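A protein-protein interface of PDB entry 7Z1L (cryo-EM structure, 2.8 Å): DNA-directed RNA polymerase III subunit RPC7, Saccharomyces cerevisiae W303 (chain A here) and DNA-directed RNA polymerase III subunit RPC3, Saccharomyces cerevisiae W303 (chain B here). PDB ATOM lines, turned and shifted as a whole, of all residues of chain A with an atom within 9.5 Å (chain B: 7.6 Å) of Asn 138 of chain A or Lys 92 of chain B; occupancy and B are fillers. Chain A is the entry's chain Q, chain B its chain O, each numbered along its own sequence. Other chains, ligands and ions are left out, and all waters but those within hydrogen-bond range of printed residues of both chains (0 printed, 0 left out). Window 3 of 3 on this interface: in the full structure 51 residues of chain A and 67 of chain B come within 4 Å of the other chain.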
ATOM      1  N   THR A  72      17.867 -12.403   9.985  1.00  0.00           N
ATOM      2  CA  THR A  72      18.855 -12.836   8.987  1.00  0.00           C
ATOM      3  C   THR A  72      19.964 -13.668   9.639  1.00  0.00           C
ATOM      4  O   THR A  72      21.119 -13.256   9.743  1.00  0.00           O
ATOM      5  CB  THR A  72      19.442 -11.650   8.209  1.00  0.00           C
ATOM      6  OG1 THR A  72      20.126 -10.760   9.100  1.00  0.00           O
ATOM      7  CG2 THR A  72      18.341 -10.892   7.487  1.00  0.00           C
ATOM      8  N   ILE A 122      10.799 -12.135   6.169  1.00  0.00           N
ATOM      9  CA  ILE A 122      11.301 -10.794   5.884  1.00  0.00           C
ATOM     10  C   ILE A 122      10.276  -9.994   5.087  1.00  0.00           C
ATOM     11  O   ILE A 122      10.124  -8.784   5.286  1.00  0.00           O
ATOM     12  CB  ILE A 122      12.665 -10.882   5.166  1.00  0.00           C
ATOM     13  CG1 ILE A 122      13.232  -9.488   4.885  1.00  0.00           C
ATOM     14  CG2 ILE A 122      12.581 -11.728   3.897  1.00  0.00           C
ATOM     15  CD1 ILE A 122      13.619  -8.726   6.124  1.00  0.00           C
ATOM     16  N   ASP A 123       9.536 -10.654   4.195  1.00  0.00           N
ATOM     17  CA  ASP A 123       8.614  -9.982   3.293  1.00  0.00           C
ATOM     18  C   ASP A 123       7.191  -9.910   3.838  1.00  0.00           C
ATOM     19  O   ASP A 123       6.248  -9.747   3.058  1.00  0.00           O
ATOM     20  CB  ASP A 123       8.620 -10.671   1.925  1.00  0.00           C
ATOM     21  CG  ASP A 123       8.362 -12.162   2.021  1.00  0.00           C
ATOM     22  OD1 ASP A 123       8.292 -12.689   3.151  1.00  0.00           O
ATOM     23  OD2 ASP A 123       8.228 -12.811   0.962  1.00  0.00           O
ATOM     24  N   TYR A 127       6.310  -2.381   4.811  1.00  0.00           N
ATOM     25  CA  TYR A 127       7.401  -1.477   4.470  1.00  0.00           C
ATOM     26  C   TYR A 127       6.891  -0.168   3.884  1.00  0.00           C
ATOM     27  O   TYR A 127       5.941  -0.145   3.095  1.00  0.00           O
ATOM     28  CB  TYR A 127       8.349  -2.144   3.475  1.00  0.00           C
ATOM     29  CG  TYR A 127       9.045  -3.374   4.001  1.00  0.00           C
ATOM     30  CD1 TYR A 127       9.622  -3.376   5.262  1.00  0.00           C
ATOM     31  CD2 TYR A 127       9.127  -4.531   3.241  1.00  0.00           C
ATOM     32  CE1 TYR A 127      10.267  -4.490   5.748  1.00  0.00           C
ATOM     33  CE2 TYR A 127       9.770  -5.652   3.719  1.00  0.00           C
ATOM     34  CZ  TYR A 127      10.336  -5.625   4.975  1.00  0.00           C
ATOM     35  OH  TYR A 127      10.979  -6.736   5.465  1.00  0.00           O
ATOM     36  N   LEU A 129       7.830   2.134   1.239  1.00  0.00           N
ATOM     37  CA  LEU A 129       8.686   1.932   0.075  1.00  0.00           C
ATOM     38  C   LEU A 129       9.497   3.170  -0.288  1.00  0.00           C
ATOM     39  O   LEU A 129      10.407   3.075  -1.119  1.00  0.00           O
ATOM     40  CB  LEU A 129       7.844   1.496  -1.124  1.00  0.00           C
ATOM     41  CG  LEU A 129       7.863   0.003  -1.453  1.00  0.00           C
ATOM     42  CD1 LEU A 129       7.214  -0.807  -0.343  1.00  0.00           C
ATOM     43  CD2 LEU A 129       7.175  -0.260  -2.783  1.00  0.00           C
ATOM     44  N   PHE A 132      13.422   2.929   0.893  1.00  0.00           N
ATOM     45  CA  PHE A 132      14.273   1.868   0.382  1.00  0.00           C
ATOM     46  C   PHE A 132      14.644   2.131  -1.069  1.00  0.00           C
ATOM     47  O   PHE A 132      13.877   2.754  -1.809  1.00  0.00           O
ATOM     48  CB  PHE A 132      13.577   0.505   0.484  1.00  0.00           C
ATOM     49  CG  PHE A 132      13.311   0.057   1.893  1.00  0.00           C
ATOM     50  CD1 PHE A 132      12.160   0.449   2.553  1.00  0.00           C
ATOM     51  CD2 PHE A 132      14.209  -0.763   2.553  1.00  0.00           C
ATOM     52  CE1 PHE A 132      11.913   0.036   3.845  1.00  0.00           C
ATOM     53  CE2 PHE A 132      13.963  -1.179   3.847  1.00  0.00           C
ATOM     54  CZ  PHE A 132      12.814  -0.779   4.492  1.00  0.00           C
ATOM     55  N   PRO A 133      15.818   1.673  -1.497  1.00  0.00           N
ATOM     56  CA  PRO A 133      16.168   1.764  -2.918  1.00  0.00           C
ATOM     57  C   PRO A 133      15.309   0.837  -3.760  1.00  0.00           C
ATOM     58  O   PRO A 133      14.743  -0.144  -3.271  1.00  0.00           O
ATOM     59  CB  PRO A 133      17.641   1.340  -2.951  1.00  0.00           C
ATOM     60  CG  PRO A 133      18.131   1.547  -1.558  1.00  0.00           C
ATOM     61  CD  PRO A 133      16.961   1.247  -0.677  1.00  0.00           C
ATOM     62  N   ASN A 134      15.213   1.168  -5.051  1.00  0.00           N
ATOM     63  CA  ASN A 134      14.343   0.421  -5.953  1.00  0.00           C
ATOM     64  C   ASN A 134      14.833  -1.004  -6.177  1.00  0.00           C
ATOM     65  O   ASN A 134      14.024  -1.901  -6.439  1.00  0.00           O
ATOM     66  CB  ASN A 134      14.225   1.152  -7.290  1.00  0.00           C
ATOM     67  CG  ASN A 134      13.316   2.362  -7.216  1.00  0.00           C
ATOM     68  OD1 ASN A 134      13.780   3.495  -7.087  1.00  0.00           O
ATOM     69  ND2 ASN A 134      12.012   2.129  -7.297  1.00  0.00           N
ATOM     70  N   GLU A 135      16.144  -1.237  -6.080  1.00  0.00           N
ATOM     71  CA  GLU A 135      16.694  -2.555  -6.373  1.00  0.00           C
ATOM     72  C   GLU A 135      16.398  -3.583  -5.289  1.00  0.00           C
ATOM     73  O   GLU A 135      16.634  -4.775  -5.514  1.00  0.00           O
ATOM     74  CB  GLU A 135      18.204  -2.458  -6.590  1.00  0.00           C
ATOM     75  CG  GLU A 135      18.999  -2.160  -5.334  1.00  0.00           C
ATOM     76  CD  GLU A 135      20.491  -2.322  -5.543  1.00  0.00           C
ATOM     77  OE1 GLU A 135      21.248  -2.191  -4.560  1.00  0.00           O
ATOM     78  OE2 GLU A 135      20.906  -2.582  -6.692  1.00  0.00           O
ATOM     79  N   LEU A 136      15.896  -3.164  -4.131  1.00  0.00           N
ATOM     80  CA  LEU A 136      15.558  -4.079  -3.051  1.00  0.00           C
ATOM     81  C   LEU A 136      14.087  -4.470  -3.040  1.00  0.00           C
ATOM     82  O   LEU A 136      13.656  -5.167  -2.117  1.00  0.00           O
ATOM     83  CB  LEU A 136      15.925  -3.460  -1.700  1.00  0.00           C
ATOM     84  CG  LEU A 136      17.380  -3.068  -1.458  1.00  0.00           C
ATOM     85  CD1 LEU A 136      17.519  -2.377  -0.114  1.00  0.00           C
ATOM     86  CD2 LEU A 136      18.278  -4.287  -1.523  1.00  0.00           C
ATOM     87  N   TYR A 137      13.308  -4.039  -4.035  1.00  0.00           N
ATOM     88  CA  TYR A 137      11.867  -4.270  -4.004  1.00  0.00           C
ATOM     89  C   TYR A 137      11.526  -5.740  -4.209  1.00  0.00           C
ATOM     90  O   TYR A 137      10.573  -6.248  -3.607  1.00  0.00           O
ATOM     91  CB  TYR A 137      11.177  -3.410  -5.063  1.00  0.00           C
ATOM     92  CG  TYR A 137      10.971  -1.968  -4.657  1.00  0.00           C
ATOM     93  CD1 TYR A 137      11.342  -1.520  -3.396  1.00  0.00           C
ATOM     94  CD2 TYR A 137      10.410  -1.055  -5.537  1.00  0.00           C
ATOM     95  CE1 TYR A 137      11.157  -0.203  -3.024  1.00  0.00           C
ATOM     96  CE2 TYR A 137      10.221   0.264  -5.173  1.00  0.00           C
ATOM     97  CZ  TYR A 137      10.597   0.683  -3.916  1.00  0.00           C
ATOM     98  OH  TYR A 137      10.411   1.995  -3.549  1.00  0.00           O
ATOM     99  N   ASN A 138      12.288  -6.440  -5.051  1.00  0.00           N
ATOM    100  CA  ASN A 138      11.919  -7.799  -5.430  1.00  0.00           C
ATOM    101  C   ASN A 138      12.107  -8.816  -4.307  1.00  0.00           C
ATOM    102  O   ASN A 138      11.495  -9.888  -4.358  1.00  0.00           O
ATOM    103  CB  ASN A 138      12.671  -8.196  -6.714  1.00  0.00           C
ATOM    104  CG  ASN A 138      14.185  -8.340  -6.528  1.00  0.00           C
ATOM    105  OD1 ASN A 138      14.680  -8.913  -5.560  1.00  0.00           O
ATOM    106  ND2 ASN A 138      14.929  -7.803  -7.489  1.00  0.00           N
ATOM    107  N   VAL A 139      12.928  -8.515  -3.296  1.00  0.00           N
ATOM    108  CA  VAL A 139      13.040  -9.410  -2.146  1.00  0.00           C
ATOM    109  C   VAL A 139      12.026  -9.091  -1.059  1.00  0.00           C
ATOM    110  O   VAL A 139      11.862  -9.891  -0.124  1.00  0.00           O
ATOM    111  CB  VAL A 139      14.455  -9.389  -1.529  1.00  0.00           C
ATOM    112  CG1 VAL A 139      15.483  -9.870  -2.537  1.00  0.00           C
ATOM    113  CG2 VAL A 139      14.798  -8.002  -1.024  1.00  0.00           C
ATOM    114  N   MET A 140      11.343  -7.953  -1.144  1.00  0.00           N
ATOM    115  CA  MET A 140      10.271  -7.630  -0.220  1.00  0.00           C
ATOM    116  C   MET A 140       8.953  -8.203  -0.733  1.00  0.00           C
ATOM    117  O   MET A 140       8.883  -8.824  -1.796  1.00  0.00           O
ATOM    118  CB  MET A 140      10.154  -6.119  -0.033  1.00  0.00           C
ATOM    119  CG  MET A 140      11.407  -5.427   0.461  1.00  0.00           C
ATOM    120  SD  MET A 140      11.148  -3.646   0.553  1.00  0.00           S
ATOM    121  CE  MET A 140      12.779  -3.038   0.166  1.00  0.00           C
ATOM    122  N   GLY A 141       7.888  -7.993   0.036  1.00  0.00           N
ATOM    123  CA  GLY A 141       6.557  -8.323  -0.427  1.00  0.00           C
ATOM    124  C   GLY A 141       5.838  -7.097  -0.947  1.00  0.00           C
ATOM    125  O   GLY A 141       5.323  -6.295  -0.162  1.00  0.00           O
ATOM    126  N   ILE A 142       5.810  -6.925  -2.267  1.00  0.00           N
ATOM    127  CA  ILE A 142       5.156  -5.754  -2.843  1.00  0.00           C
ATOM    128  C   ILE A 142       3.642  -5.867  -2.707  1.00  0.00           C
ATOM    129  O   ILE A 142       2.965  -4.916  -2.298  1.00  0.00           O
ATOM    130  CB  ILE A 142       5.585  -5.568  -4.309  1.00  0.00           C
ATOM    131  CG1 ILE A 142       7.081  -5.257  -4.387  1.00  0.00           C
ATOM    132  CG2 ILE A 142       4.779  -4.459  -4.971  1.00  0.00           C
ATOM    133  CD1 ILE A 142       7.631  -5.257  -5.795  1.00  0.00           C
ATOM    134  N   ASN A 143       3.090  -7.033  -3.030  1.00  0.00           N
ATOM    135  CA  ASN A 143       1.643  -7.226  -3.072  1.00  0.00           C
ATOM    136  C   ASN A 143       1.250  -8.546  -2.411  1.00  0.00           C
ATOM    137  O   ASN A 143       0.472  -9.332  -2.951  1.00  0.00           O
ATOM    138  CB  ASN A 143       1.138  -7.148  -4.513  1.00  0.00           C
ATOM    139  CG  ASN A 143       1.888  -8.081  -5.450  1.00  0.00           C
ATOM    140  OD1 ASN A 143       2.746  -8.855  -5.027  1.00  0.00           O
ATOM    141  ND2 ASN A 143       1.562  -8.008  -6.736  1.00  0.00           N
ATOM    142  N   LYS A 144       1.786  -8.804  -1.223  1.00  0.00           N
ATOM    143  CA  LYS A 144       1.472 -10.015  -0.475  1.00  0.00           C
ATOM    144  C   LYS A 144       0.934  -9.651   0.909  1.00  0.00           C
ATOM    145  O   LYS A 144       0.831  -8.477   1.272  1.00  0.00           O
ATOM    146  CB  LYS A 144       2.696 -10.930  -0.380  1.00  0.00           C
ATOM    147  CG  LYS A 144       3.724 -10.523   0.659  1.00  0.00           C
ATOM    148  CD  LYS A 144       4.844 -11.547   0.741  1.00  0.00           C
ATOM    149  CE  LYS A 144       4.309 -12.927   1.088  1.00  0.00           C
ATOM    150  NZ  LYS A 144       3.410 -12.897   2.275  1.00  0.00           N
ATOM    151  N   ARG B  60      24.768 -12.754   9.163  1.00  0.00           N
ATOM    152  CA  ARG B  60      24.848 -12.187   7.818  1.00  0.00           C
ATOM    153  C   ARG B  60      24.859 -10.664   7.860  1.00  0.00           C
ATOM    154  O   ARG B  60      25.641 -10.017   7.148  1.00  0.00           O
ATOM    155  CB  ARG B  60      23.683 -12.696   6.974  1.00  0.00           C
ATOM    156  CG  ARG B  60      23.950 -14.025   6.292  1.00  0.00           C
ATOM    157  CD  ARG B  60      22.680 -14.840   6.140  1.00  0.00           C
ATOM    158  NE  ARG B  60      21.771 -14.279   5.150  1.00  0.00           N
ATOM    159  CZ  ARG B  60      20.498 -14.626   5.025  1.00  0.00           C
ATOM    160  NH1 ARG B  60      19.947 -15.530   5.818  1.00  0.00           N
ATOM    161  NH2 ARG B  60      19.759 -14.052   4.081  1.00  0.00           N
ATOM    162  N   VAL B  64      27.840  -8.086   6.673  1.00  0.00           N
ATOM    163  CA  VAL B  64      27.618  -6.945   5.786  1.00  0.00           C
ATOM    164  C   VAL B  64      28.104  -5.654   6.439  1.00  0.00           C
ATOM    165  O   VAL B  64      28.797  -4.845   5.809  1.00  0.00           O
ATOM    166  CB  VAL B  64      26.137  -6.860   5.380  1.00  0.00           C
ATOM    167  CG1 VAL B  64      25.814  -5.495   4.801  1.00  0.00           C
ATOM    168  CG2 VAL B  64      25.817  -7.942   4.371  1.00  0.00           C
ATOM    169  N   VAL B  76      25.822  -3.456  -4.122  1.00  0.00           N
ATOM    170  CA  VAL B  76      25.323  -4.798  -3.838  1.00  0.00           C
ATOM    171  C   VAL B  76      26.172  -5.844  -4.556  1.00  0.00           C
ATOM    172  O   VAL B  76      26.461  -6.913  -4.006  1.00  0.00           O
ATOM    173  CB  VAL B  76      23.826  -4.904  -4.197  1.00  0.00           C
ATOM    174  CG1 VAL B  76      23.564  -4.481  -5.639  1.00  0.00           C
ATOM    175  CG2 VAL B  76      23.306  -6.311  -3.942  1.00  0.00           C
ATOM    176  N   VAL B  80      28.421  -8.700  -2.823  1.00  0.00           N
ATOM    177  CA  VAL B  80      28.312 -10.108  -3.199  1.00  0.00           C
ATOM    178  C   VAL B  80      29.692 -10.688  -3.483  1.00  0.00           C
ATOM    179  O   VAL B  80      30.051 -11.760  -2.981  1.00  0.00           O
ATOM    180  CB  VAL B  80      27.375 -10.269  -4.409  1.00  0.00           C
ATOM    181  CG1 VAL B  80      27.580 -11.621  -5.074  1.00  0.00           C
ATOM    182  CG2 VAL B  80      25.935 -10.110  -3.981  1.00  0.00           C
ATOM    183  N   MET B  86      27.587 -15.827   0.096  1.00  0.00           N
ATOM    184  CA  MET B  86      26.336 -15.081   0.086  1.00  0.00           C
ATOM    185  C   MET B  86      26.050 -14.602  -1.329  1.00  0.00           C
ATOM    186  O   MET B  86      26.881 -13.923  -1.939  1.00  0.00           O
ATOM    187  CB  MET B  86      26.401 -13.899   1.058  1.00  0.00           C
ATOM    188  CG  MET B  86      26.347 -14.322   2.519  1.00  0.00           C
ATOM    189  SD  MET B  86      26.244 -12.969   3.706  1.00  0.00           S
ATOM    190  CE  MET B  86      25.146 -11.843   2.861  1.00  0.00           C
ATOM    191  N   ASP B  87      24.876 -14.958  -1.846  1.00  0.00           N
ATOM    192  CA  ASP B  87      24.477 -14.571  -3.188  1.00  0.00           C
ATOM    193  C   ASP B  87      23.724 -13.241  -3.161  1.00  0.00           C
ATOM    194  O   ASP B  87      23.604 -12.588  -2.123  1.00  0.00           O
ATOM    195  CB  ASP B  87      23.664 -15.689  -3.847  1.00  0.00           C
ATOM    196  CG  ASP B  87      22.360 -15.997  -3.118  1.00  0.00           C
ATOM    197  OD1 ASP B  87      22.073 -15.388  -2.065  1.00  0.00           O
ATOM    198  OD2 ASP B  87      21.608 -16.862  -3.614  1.00  0.00           O
ATOM    199  N   VAL B  88      23.206 -12.837  -4.324  1.00  0.00           N
ATOM    200  CA  VAL B  88      22.592 -11.518  -4.449  1.00  0.00           C
ATOM    201  C   VAL B  88      21.293 -11.444  -3.650  1.00  0.00           C
ATOM    202  O   VAL B  88      20.974 -10.406  -3.055  1.00  0.00           O
ATOM    203  CB  VAL B  88      22.394 -11.160  -5.938  1.00  0.00           C
ATOM    204  CG1 VAL B  88      21.480 -12.154  -6.644  1.00  0.00           C
ATOM    205  CG2 VAL B  88      21.876  -9.736  -6.088  1.00  0.00           C
ATOM    206  N   ASP B  89      20.537 -12.546  -3.599  1.00  0.00           N
ATOM    207  CA  ASP B  89      19.277 -12.544  -2.861  1.00  0.00           C
ATOM    208  C   ASP B  89      19.509 -12.405  -1.363  1.00  0.00           C
ATOM    209  O   ASP B  89      18.808 -11.642  -0.688  1.00  0.00           O
ATOM    210  CB  ASP B  89      18.492 -13.819  -3.167  1.00  0.00           C
ATOM    211  CG  ASP B  89      17.983 -13.858  -4.594  1.00  0.00           C
ATOM    212  OD1 ASP B  89      17.647 -12.784  -5.135  1.00  0.00           O
ATOM    213  OD2 ASP B  89      17.919 -14.962  -5.175  1.00  0.00           O
ATOM    214  N   SER B  90      20.494 -13.130  -0.826  1.00  0.00           N
ATOM    215  CA  SER B  90      20.795 -13.038   0.600  1.00  0.00           C
ATOM    216  C   SER B  90      21.313 -11.653   0.969  1.00  0.00           C
ATOM    217  O   SER B  90      20.933 -11.099   2.010  1.00  0.00           O
ATOM    218  CB  SER B  90      21.808 -14.111   0.989  1.00  0.00           C
ATOM    219  OG  SER B  90      22.035 -14.112   2.386  1.00  0.00           O
ATOM    220  N   VAL B  91      22.179 -11.081   0.127  1.00  0.00           N
ATOM    221  CA  VAL B  91      22.699  -9.739   0.377  1.00  0.00           C
ATOM    222  C   VAL B  91      21.571  -8.718   0.352  1.00  0.00           C
ATOM    223  O   VAL B  91      21.497  -7.836   1.213  1.00  0.00           O
ATOM    224  CB  VAL B  91      23.803  -9.390  -0.640  1.00  0.00           C
ATOM    225  CG1 VAL B  91      24.180  -7.924  -0.538  1.00  0.00           C
ATOM    226  CG2 VAL B  91      25.025 -10.247  -0.405  1.00  0.00           C
ATOM    227  N   LYS B  92      20.665  -8.830  -0.622  1.00  0.00           N
ATOM    228  CA  LYS B  92      19.547  -7.894  -0.696  1.00  0.00           C
ATOM    229  C   LYS B  92      18.609  -8.047   0.497  1.00  0.00           C
ATOM    230  O   LYS B  92      18.116  -7.048   1.033  1.00  0.00           O
ATOM    231  CB  LYS B  92      18.799  -8.086  -2.014  1.00  0.00           C
ATOM    232  CG  LYS B  92      19.459  -7.375  -3.183  1.00  0.00           C
ATOM    233  CD  LYS B  92      18.544  -7.297  -4.386  1.00  0.00           C
ATOM    234  CE  LYS B  92      18.415  -8.650  -5.056  1.00  0.00           C
ATOM    235  NZ  LYS B  92      17.577  -8.582  -6.280  1.00  0.00           N
ATOM    236  N   THR B  93      18.370  -9.284   0.942  1.00  0.00           N
ATOM    237  CA  THR B  93      17.499  -9.509   2.092  1.00  0.00           C
ATOM    238  C   THR B  93      18.096  -8.918   3.365  1.00  0.00           C
ATOM    239  O   THR B  93      17.407  -8.226   4.128  1.00  0.00           O
ATOM    240  CB  THR B  93      17.240 -11.005   2.268  1.00  0.00           C
ATOM    241  OG1 THR B  93      16.617 -11.524   1.087  1.00  0.00           O
ATOM    242  CG2 THR B  93      16.333 -11.253   3.461  1.00  0.00           C
ATOM    243  N   THR B  94      19.386  -9.169   3.611  1.00  0.00           N
ATOM    244  CA  THR B  94      19.991  -8.619   4.820  1.00  0.00           C
ATOM    245  C   THR B  94      20.177  -7.110   4.715  1.00  0.00           C
ATOM    246  O   THR B  94      20.166  -6.417   5.737  1.00  0.00           O
ATOM    247  CB  THR B  94      21.317  -9.319   5.134  1.00  0.00           C
ATOM    248  OG1 THR B  94      21.820  -8.838   6.385  1.00  0.00           O
ATOM    249  CG2 THR B  94      22.348  -9.059   4.063  1.00  0.00           C
ATOM    250  N   LEU B  95      20.296  -6.574   3.496  1.00  0.00           N
ATOM    251  CA  LEU B  95      20.326  -5.126   3.333  1.00  0.00           C
ATOM    252  C   LEU B  95      18.972  -4.511   3.651  1.00  0.00           C
ATOM    253  O   LEU B  95      18.904  -3.433   4.244  1.00  0.00           O
ATOM    254  CB  LEU B  95      20.764  -4.759   1.917  1.00  0.00           C
ATOM    255  CG  LEU B  95      22.270  -4.665   1.686  1.00  0.00           C
ATOM    256  CD1 LEU B  95      22.576  -4.622   0.202  1.00  0.00           C
ATOM    257  CD2 LEU B  95      22.845  -3.452   2.389  1.00  0.00           C
ATOM    258  N   VAL B  96      17.885  -5.185   3.268  1.00  0.00           N
ATOM    259  CA  VAL B  96      16.547  -4.730   3.647  1.00  0.00           C
ATOM    260  C   VAL B  96      16.390  -4.759   5.162  1.00  0.00           C
ATOM    261  O   VAL B  96      15.870  -3.814   5.774  1.00  0.00           O
ATOM    262  CB  VAL B  96      15.474  -5.590   2.953  1.00  0.00           C
ATOM    263  CG1 VAL B  96      14.114  -5.386   3.599  1.00  0.00           C
ATOM    264  CG2 VAL B  96      15.413  -5.263   1.478  1.00  0.00           C
ATOM    265  N   SER B  97      16.854  -5.844   5.788  1.00  0.00           N
ATOM    266  CA  SER B  97      16.756  -5.973   7.240  1.00  0.00           C
ATOM    267  C   SER B  97      17.549  -4.886   7.956  1.00  0.00           C
ATOM    268  O   SER B  97      17.095  -4.340   8.968  1.00  0.00           O
ATOM    269  CB  SER B  97      17.233  -7.357   7.674  1.00  0.00           C
ATOM    270  OG  SER B  97      17.353  -7.439   9.082  1.00  0.00           O
ATOM    271  N   LEU B  98      18.739  -4.560   7.449  1.00  0.00           N
ATOM    272  CA  LEU B  98      19.532  -3.490   8.045  1.00  0.00           C
ATOM    273  C   LEU B  98      18.919  -2.121   7.775  1.00  0.00           C
ATOM    274  O   LEU B  98      18.984  -1.227   8.627  1.00  0.00           O
ATOM    275  CB  LEU B  98      20.963  -3.545   7.518  1.00  0.00           C
ATOM    276  CG  LEU B  98      21.862  -4.633   8.098  1.00  0.00           C
ATOM    277  CD1 LEU B  98      23.032  -4.889   7.173  1.00  0.00           C
ATOM    278  CD2 LEU B  98      22.348  -4.234   9.474  1.00  0.00           C
ATOM    279  N   THR B  99      18.329  -1.934   6.592  1.00  0.00           N
ATOM    280  CA  THR B  99      17.764  -0.641   6.226  1.00  0.00           C
ATOM    281  C   THR B  99      16.524  -0.325   7.050  1.00  0.00           C
ATOM    282  O   THR B  99      16.268   0.840   7.373  1.00  0.00           O
ATOM    283  CB  THR B  99      17.436  -0.622   4.732  1.00  0.00           C
ATOM    284  OG1 THR B  99      18.515  -1.213   3.999  1.00  0.00           O
ATOM    285  CG2 THR B  99      17.228   0.797   4.240  1.00  0.00           C
ATOM    286  N   TYR B 120      25.702   1.556  -0.628  1.00  0.00           N
ATOM    287  CA  TYR B 120      25.210   1.468   0.739  1.00  0.00           C
ATOM    288  C   TYR B 120      26.337   1.814   1.699  1.00  0.00           C
ATOM    289  O   TYR B 120      27.457   1.315   1.551  1.00  0.00           O
ATOM    290  CB  TYR B 120      24.673   0.069   1.039  1.00  0.00           C
ATOM    291  CG  TYR B 120      23.454  -0.298   0.232  1.00  0.00           C
ATOM    292  CD1 TYR B 120      23.579  -0.839  -1.037  1.00  0.00           C
ATOM    293  CD2 TYR B 120      22.178  -0.097   0.735  1.00  0.00           C
ATOM    294  CE1 TYR B 120      22.472  -1.173  -1.783  1.00  0.00           C
ATOM    295  CE2 TYR B 120      21.062  -0.426  -0.004  1.00  0.00           C
ATOM    296  CZ  TYR B 120      21.216  -0.963  -1.263  1.00  0.00           C
ATOM    297  OH  TYR B 120      20.111  -1.298  -2.007  1.00  0.00           O
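NE of Arg 60 of chain B lies within hydrogen-bond range of OG of Ser 90 of chain B, 2.8 Å away. The backbone carbonyl oxygen (O) of Asp 89 of chain B lies within hydrogen-bond range of the side-chain hydroxyl (OG1) of Thr 93 of chain B, 2.8 Å away.
N of Arg 60 of chain B touches O of Thr 72 of chain A, 3.7 Å away. Thr 94 of chain B touches Thr 72 of chain A. Tyr 127 of chain A touches Val 96 of chain B (OH to CG1, 3.9 Å). O of Val 96 of chain B touches CE2 of Phe 132 of chain A (3.8 Å). Thr 99 of chain B touches Phe 132 of chain A (CB to CE2, 3.6 Å). Tyr 120 of chain B touches Pro 133 of chain A (OH to CG, 3.5 Å). Lys 92 of chain B touches Leu 136 of chain A (CG to CD2, 3.7 Å). Tyr 120 of chain B touches Leu 136 of chain A. Val 139 of chain A touches Lys 92 of chain B (CG1 to CB, 3.8 Å). Met 140 of chain A touches Val 96 of chain B (CE to CG2, 3.7 Å).
The side-chain amino group (NZ) of Lys 92 of chain B lies within hydrogen-bond range of the side-chain amide oxygen (OD1) of Asn 138 of chain A, 3.0 Å away. The side-chain hydroxyl (OH) of Tyr 120 of chain B sits at hydrogen-bond distance from the side-chain carboxylate (OE1) of Glu 135 of chain A (2.9 Å).
Of the 18 printed residues of chain A, 10 touch a printed residue of chain B. Printed residues of chain A that touch a printed residue of chain B: Thr 72, Ile 122, Tyr 127, Phe 132, Pro 133, Glu 135, Leu 136, Asn 138, Val 139 and Met 140. Hydrophobic or aromatic side chains of chain A within 4 Å of the printed part of chain B: Ile 122, Tyr 127, Phe 132, Pro 133, Leu 136, Val 139 and Met 140. Printed residues of chain B that touch a printed residue of chain A: Arg 60, Val 76, Lys 92, Thr 93, Thr 94, Val 96, Ser 97, Thr 99 and Tyr 120. Hydrophobic or aromatic side chains of chain B that line the printed part of chain A: Val 76, Val 96 and Tyr 120. Among the printed residues, 18 pairs touch across the chains. Among the printed residues, no Asp or Glu carboxylate lies within 4 Å of a Lys or Arg side-chain nitrogen of the other chain.
Lys 92 of chain B touches four residues of chain A. No residue of chain A comes within 4 Å of Val 91 of chain B. Of the printed residues of chain A, Val 96 of chain B touches Tyr 127, Phe 132, Leu 136, Val 139 and Met 140. Printed residues of chain B within 4 Å of Ile 122 of chain A: Thr 93. Ser 90 of chain B touches none of the printed residues of chain A. The nearest residue of chain B that does not touch Asn 138 of chain A is Asp 89 of chain B (4.9 Å). The nearest residue of chain A that does not touch Lys 92 of chain B is Tyr 137 of chain A (6.2 Å). The nearest printed residue of chain A that does not touch Arg 60 of chain B is Ile 122 of chain A (7.5 Å).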
